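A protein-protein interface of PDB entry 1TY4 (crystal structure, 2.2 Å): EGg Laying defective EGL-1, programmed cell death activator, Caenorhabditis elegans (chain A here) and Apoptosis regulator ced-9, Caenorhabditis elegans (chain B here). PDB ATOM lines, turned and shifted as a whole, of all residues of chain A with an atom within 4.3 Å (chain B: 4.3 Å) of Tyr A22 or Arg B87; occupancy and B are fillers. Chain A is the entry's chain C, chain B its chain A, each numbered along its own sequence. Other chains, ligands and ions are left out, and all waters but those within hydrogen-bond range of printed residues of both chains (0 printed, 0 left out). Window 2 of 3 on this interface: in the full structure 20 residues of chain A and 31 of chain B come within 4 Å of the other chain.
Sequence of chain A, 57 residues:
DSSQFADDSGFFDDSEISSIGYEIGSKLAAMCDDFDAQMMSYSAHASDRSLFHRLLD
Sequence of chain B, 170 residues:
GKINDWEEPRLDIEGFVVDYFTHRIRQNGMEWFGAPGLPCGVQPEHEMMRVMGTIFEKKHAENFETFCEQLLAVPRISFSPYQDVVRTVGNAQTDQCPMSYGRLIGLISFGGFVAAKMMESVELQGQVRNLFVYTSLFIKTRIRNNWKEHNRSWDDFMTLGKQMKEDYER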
ATOM      1  N   SER A  19      24.865  19.590 -24.311  1.00  0.00           N
ATOM      2  CA  SER A  19      23.681  19.086 -24.998  1.00  0.00           C
ATOM      3  C   SER A  19      22.522  19.775 -24.284  1.00  0.00           C
ATOM      4  O   SER A  19      21.460  20.008 -24.863  1.00  0.00           O
ATOM      5  CB  SER A  19      23.595  17.555 -24.869  1.00  0.00           C
ATOM      6  OG  SER A  19      22.282  17.106 -24.579  1.00  0.00           O
ATOM      7  N   ILE A  20      22.760  20.128 -23.021  1.00  0.00           N
ATOM      8  CA  ILE A  20      21.764  20.793 -22.203  1.00  0.00           C
ATOM      9  C   ILE A  20      21.487  22.200 -22.738  1.00  0.00           C
ATOM     10  O   ILE A  20      20.362  22.661 -22.703  1.00  0.00           O
ATOM     11  CB  ILE A  20      22.213  20.878 -20.725  1.00  0.00           C
ATOM     12  CG1 ILE A  20      21.030  21.291 -19.854  1.00  0.00           C
ATOM     13  CG2 ILE A  20      23.341  21.896 -20.553  1.00  0.00           C
ATOM     14  CD1 ILE A  20      19.971  20.225 -19.735  1.00  0.00           C
ATOM     15  N   GLY A  21      22.517  22.870 -23.242  1.00  0.00           N
ATOM     16  CA  GLY A  21      22.334  24.203 -23.785  1.00  0.00           C
ATOM     17  C   GLY A  21      21.421  24.177 -24.993  1.00  0.00           C
ATOM     18  O   GLY A  21      20.608  25.075 -25.194  1.00  0.00           O
ATOM     19  N   TYR A  22      21.540  23.135 -25.802  1.00  0.00           N
ATOM     20  CA  TYR A  22      20.697  23.022 -26.985  1.00  0.00           C
ATOM     21  C   TYR A  22      19.235  22.826 -26.609  1.00  0.00           C
ATOM     22  O   TYR A  22      18.351  23.422 -27.225  1.00  0.00           O
ATOM     23  CB  TYR A  22      21.163  21.869 -27.875  1.00  0.00           C
ATOM     24  CG  TYR A  22      22.547  22.074 -28.456  1.00  0.00           C
ATOM     25  CD1 TYR A  22      23.687  21.647 -27.769  1.00  0.00           C
ATOM     26  CD2 TYR A  22      22.721  22.708 -29.690  1.00  0.00           C
ATOM     27  CE1 TYR A  22      24.966  21.844 -28.299  1.00  0.00           C
ATOM     28  CE2 TYR A  22      23.996  22.912 -30.228  1.00  0.00           C
ATOM     29  CZ  TYR A  22      25.112  22.476 -29.528  1.00  0.00           C
ATOM     30  OH  TYR A  22      26.369  22.659 -30.062  1.00  0.00           O
ATOM     31  N   GLU A  23      18.967  22.014 -25.593  1.00  0.00           N
ATOM     32  CA  GLU A  23      17.579  21.793 -25.217  1.00  0.00           C
ATOM     33  C   GLU A  23      17.032  22.989 -24.447  1.00  0.00           C
ATOM     34  O   GLU A  23      15.858  23.332 -24.584  1.00  0.00           O
ATOM     35  CB  GLU A  23      17.417  20.490 -24.418  1.00  0.00           C
ATOM     36  CG  GLU A  23      17.597  20.589 -22.924  1.00  0.00           C
ATOM     37  CD  GLU A  23      17.124  19.328 -22.208  1.00  0.00           C
ATOM     38  OE1 GLU A  23      17.629  18.227 -22.538  1.00  0.00           O
ATOM     39  OE2 GLU A  23      16.249  19.437 -21.318  1.00  0.00           O
ATOM     40  N   ILE A  24      17.870  23.634 -23.639  1.00  0.00           N
ATOM     41  CA  ILE A  24      17.394  24.816 -22.928  1.00  0.00           C
ATOM     42  C   ILE A  24      17.077  25.863 -24.002  1.00  0.00           C
ATOM     43  O   ILE A  24      16.071  26.567 -23.928  1.00  0.00           O
ATOM     44  CB  ILE A  24      18.465  25.404 -21.974  1.00  0.00           C
ATOM     45  CG1 ILE A  24      18.554  24.567 -20.696  1.00  0.00           C
ATOM     46  CG2 ILE A  24      18.122  26.843 -21.631  1.00  0.00           C
ATOM     47  CD1 ILE A  24      19.661  25.011 -19.759  1.00  0.00           C
ATOM     48  N   GLY A  25      17.944  25.937 -25.008  1.00  0.00           N
ATOM     49  CA  GLY A  25      17.759  26.901 -26.080  1.00  0.00           C
ATOM     50  C   GLY A  25      16.500  26.666 -26.890  1.00  0.00           C
ATOM     51  O   GLY A  25      15.832  27.621 -27.304  1.00  0.00           O
ATOM     52  N   SER A  26      16.178  25.398 -27.129  1.00  0.00           N
ATOM     53  CA  SER A  26      14.982  25.051 -27.893  1.00  0.00           C
ATOM     54  C   SER A  26      13.747  25.547 -27.176  1.00  0.00           C
ATOM     55  O   SER A  26      12.814  26.023 -27.810  1.00  0.00           O
ATOM     56  CB  SER A  26      14.880  23.539 -28.083  1.00  0.00           C
ATOM     57  OG  SER A  26      15.933  23.085 -28.908  1.00  0.00           O
ATOM     58  N   GLN B  83      26.449  29.529 -24.294  1.00  0.00           N
ATOM     59  CA  GLN B  83      26.592  30.000 -25.664  1.00  0.00           C
ATOM     60  C   GLN B  83      25.703  29.117 -26.528  1.00  0.00           C
ATOM     61  O   GLN B  83      25.072  29.599 -27.462  1.00  0.00           O
ATOM     62  CB  GLN B  83      28.056  29.921 -26.115  1.00  0.00           C
ATOM     63  CG  GLN B  83      28.946  30.920 -25.389  1.00  0.00           C
ATOM     64  CD  GLN B  83      30.412  30.792 -25.748  1.00  0.00           C
ATOM     65  OE1 GLN B  83      30.973  29.701 -25.706  1.00  0.00           O
ATOM     66  NE2 GLN B  83      31.044  31.910 -26.085  1.00  0.00           N
ATOM     67  N   ASP B  84      25.634  27.827 -26.202  1.00  0.00           N
ATOM     68  CA  ASP B  84      24.779  26.911 -26.956  1.00  0.00           C
ATOM     69  C   ASP B  84      23.323  27.365 -26.842  1.00  0.00           C
ATOM     70  O   ASP B  84      22.562  27.268 -27.804  1.00  0.00           O
ATOM     71  CB  ASP B  84      24.905  25.470 -26.440  1.00  0.00           C
ATOM     72  CG  ASP B  84      26.273  24.854 -26.726  1.00  0.00           C
ATOM     73  OD1 ASP B  84      26.931  25.241 -27.722  1.00  0.00           O
ATOM     74  OD2 ASP B  84      26.685  23.965 -25.958  1.00  0.00           O
ATOM     75  N   VAL B  85      22.933  27.851 -25.663  1.00  0.00           N
ATOM     76  CA  VAL B  85      21.570  28.329 -25.481  1.00  0.00           C
ATOM     77  C   VAL B  85      21.305  29.473 -26.457  1.00  0.00           C
ATOM     78  O   VAL B  85      20.388  29.414 -27.283  1.00  0.00           O
ATOM     79  CB  VAL B  85      21.320  28.901 -24.062  1.00  0.00           C
ATOM     80  CG1 VAL B  85      19.964  29.612 -24.038  1.00  0.00           C
ATOM     81  CG2 VAL B  85      21.351  27.798 -23.033  1.00  0.00           C
ATOM     82  N   VAL B  86      22.118  30.519 -26.338  1.00  0.00           N
ATOM     83  CA  VAL B  86      21.985  31.702 -27.167  1.00  0.00           C
ATOM     84  C   VAL B  86      22.042  31.418 -28.665  1.00  0.00           C
ATOM     85  O   VAL B  86      21.218  31.921 -29.427  1.00  0.00           O
ATOM     86  CB  VAL B  86      23.073  32.746 -26.806  1.00  0.00           C
ATOM     87  CG1 VAL B  86      23.040  33.902 -27.805  1.00  0.00           C
ATOM     88  CG2 VAL B  86      22.848  33.262 -25.375  1.00  0.00           C
ATOM     89  N   ARG B  87      23.012  30.614 -29.084  1.00  0.00           N
ATOM     90  CA  ARG B  87      23.165  30.293 -30.499  1.00  0.00           C
ATOM     91  C   ARG B  87      21.942  29.543 -31.007  1.00  0.00           C
ATOM     92  O   ARG B  87      21.486  29.770 -32.128  1.00  0.00           O
ATOM     93  CB  ARG B  87      24.414  29.440 -30.721  1.00  0.00           C
ATOM     94  CG  ARG B  87      24.957  29.505 -32.143  1.00  0.00           C
ATOM     95  CD  ARG B  87      25.999  28.431 -32.400  1.00  0.00           C
ATOM     96  NE  ARG B  87      26.909  28.284 -31.274  1.00  0.00           N
ATOM     97  CZ  ARG B  87      26.956  27.210 -30.493  1.00  0.00           C
ATOM     98  NH1 ARG B  87      26.149  26.189 -30.726  1.00  0.00           N
ATOM     99  NH2 ARG B  87      27.804  27.163 -29.473  1.00  0.00           N
ATOM    100  N   THR B  88      21.405  28.657 -30.172  1.00  0.00           N
ATOM    101  CA  THR B  88      20.246  27.872 -30.551  1.00  0.00           C
ATOM    102  C   THR B  88      19.035  28.766 -30.760  1.00  0.00           C
ATOM    103  O   THR B  88      18.260  28.554 -31.693  1.00  0.00           O
ATOM    104  CB  THR B  88      19.923  26.796 -29.488  1.00  0.00           C
ATOM    105  OG1 THR B  88      20.992  25.841 -29.434  1.00  0.00           O
ATOM    106  CG2 THR B  88      18.622  26.067 -29.827  1.00  0.00           C
ATOM    107  N   VAL B  89      18.863  29.770 -29.907  1.00  0.00           N
ATOM    108  CA  VAL B  89      17.718  30.662 -30.059  1.00  0.00           C
ATOM    109  C   VAL B  89      17.816  31.421 -31.377  1.00  0.00           C
ATOM    110  O   VAL B  89      16.829  31.559 -32.099  1.00  0.00           O
ATOM    111  CB  VAL B  89      17.623  31.677 -28.909  1.00  0.00           C
ATOM    112  CG1 VAL B  89      16.639  32.783 -29.278  1.00  0.00           C
ATOM    113  CG2 VAL B  89      17.159  30.976 -27.634  1.00  0.00           C
ATOM    114  N   GLY B  90      19.012  31.906 -31.685  1.00  0.00           N
ATOM    115  CA  GLY B  90      19.217  32.645 -32.916  1.00  0.00           C
ATOM    116  C   GLY B  90      19.101  31.815 -34.182  1.00  0.00           C
ATOM    117  O   GLY B  90      18.807  32.365 -35.249  1.00  0.00           O
ATOM    118  N   ASN B  91      19.333  30.503 -34.076  1.00  0.00           N
ATOM    119  CA  ASN B  91      19.250  29.621 -35.237  1.00  0.00           C
ATOM    120  C   ASN B  91      18.044  28.741 -35.221  1.00  0.00           C
ATOM    121  O   ASN B  91      17.898  27.873 -36.100  1.00  0.00           O
ATOM    122  CB  ASN B  91      20.471  28.730 -35.375  1.00  0.00           C
ATOM    123  CG  ASN B  91      21.755  29.501 -35.323  1.00  0.00           C
ATOM    124  OD1 ASN B  91      21.809  30.695 -35.639  1.00  0.00           O
ATOM    125  ND2 ASN B  91      22.817  28.816 -34.929  1.00  0.00           N
ATOM    126  N   TYR B 134      29.463  38.501 -24.571  1.00  0.00           N
ATOM    127  CA  TYR B 134      29.003  37.522 -25.543  1.00  0.00           C
ATOM    128  C   TYR B 134      27.550  37.717 -25.968  1.00  0.00           C
ATOM    129  O   TYR B 134      27.222  37.599 -27.150  1.00  0.00           O
ATOM    130  CB  TYR B 134      29.151  36.106 -24.995  1.00  0.00           C
ATOM    131  CG  TYR B 134      28.565  35.094 -25.936  1.00  0.00           C
ATOM    132  CD1 TYR B 134      29.272  34.663 -27.055  1.00  0.00           C
ATOM    133  CD2 TYR B 134      27.271  34.614 -25.749  1.00  0.00           C
ATOM    134  CE1 TYR B 134      28.700  33.776 -27.965  1.00  0.00           C
ATOM    135  CE2 TYR B 134      26.691  33.735 -26.651  1.00  0.00           C
ATOM    136  CZ  TYR B 134      27.407  33.318 -27.753  1.00  0.00           C
ATOM    137  OH  TYR B 134      26.830  32.434 -28.641  1.00  0.00           O
ATOM    138  N   PHE B 138      26.683  38.630 -29.804  1.00  0.00           N
ATOM    139  CA  PHE B 138      25.890  37.706 -30.583  1.00  0.00           C
ATOM    140  C   PHE B 138      24.678  38.424 -31.152  1.00  0.00           C
ATOM    141  O   PHE B 138      24.420  38.366 -32.348  1.00  0.00           O
ATOM    142  CB  PHE B 138      25.451  36.506 -29.738  1.00  0.00           C
ATOM    143  CG  PHE B 138      24.611  35.525 -30.499  1.00  0.00           C
ATOM    144  CD1 PHE B 138      23.231  35.688 -30.571  1.00  0.00           C
ATOM    145  CD2 PHE B 138      25.207  34.488 -31.213  1.00  0.00           C
ATOM    146  CE1 PHE B 138      22.453  34.835 -31.346  1.00  0.00           C
ATOM    147  CE2 PHE B 138      24.439  33.630 -31.993  1.00  0.00           C
ATOM    148  CZ  PHE B 138      23.058  33.804 -32.062  1.00  0.00           C
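O of Asp B84 sits at hydrogen-bond distance from OG1 of Thr B88, 2.7 Å away.
The backbone carbonyl oxygen of Arg B87 sits close to the side-chain amide nitrogen of Asn B91 (3.2 Å).
The guanidinium group of Arg B87 lies within salt-bridge range of the side-chain carboxylate of Asp B84, 2.7 Å away.
O of Tyr A22 sits at hydrogen-bond distance from OG of Ser A26 (3.0 Å).
Asp B84 touches Gly A21.
O of Gly A21 touches CA of Val B85 (3.4 Å).
Tyr A22 touches Asp B84.
Arg B87 touches Tyr A22.
Tyr A22 touches Thr B88 (CD2 to OG1, 3.6 Å).
CG2 of Val B85 touches CG2 of Ile A24, at 3.6 Å.
Gly A25 touches Val B85 (CA to O, 3.8 Å).
CG2 of Thr B88 touches C of Gly A25 (3.7 Å).
Gly A25 touches Val B89.
CG2 of Thr B88 touches N of Ser A26, at 3.7 Å.
Of chain B, only Asp B84, Arg B87 and Thr B88 come within 4 Å of Tyr A22.
Of chain A, only Tyr A22 (3.6 Å) comes within 4 Å of Arg B87.
Of the printed residues of chain B, Gly A21 touches Asp B84 (3.9 Å) and Val B85 (3.4 Å).
Printed residues of chain B within 4 Å of Ser A26: Thr B88.
Ile A20 touches none of the printed residues of chain B.
Val B86 touches none of the printed residues of chain A.
The nearest printed residue of chain B that does not touch Tyr A22 is Val B85 (4.9 Å).
The nearest printed residue of chain A that does not touch Arg B87 is Gly A25 (7.0 Å).
Hydrophobic or aromatic side chains of chain A that line the printed part of chain B: Tyr A22 and Ile A24.
Of the 11 printed residues of chain B, 5 touch a printed residue of chain A.
Among the printed residues, no Asp or Glu carboxylate lies within 4 Å of a Lys or Arg side-chain nitrogen of the other chain.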
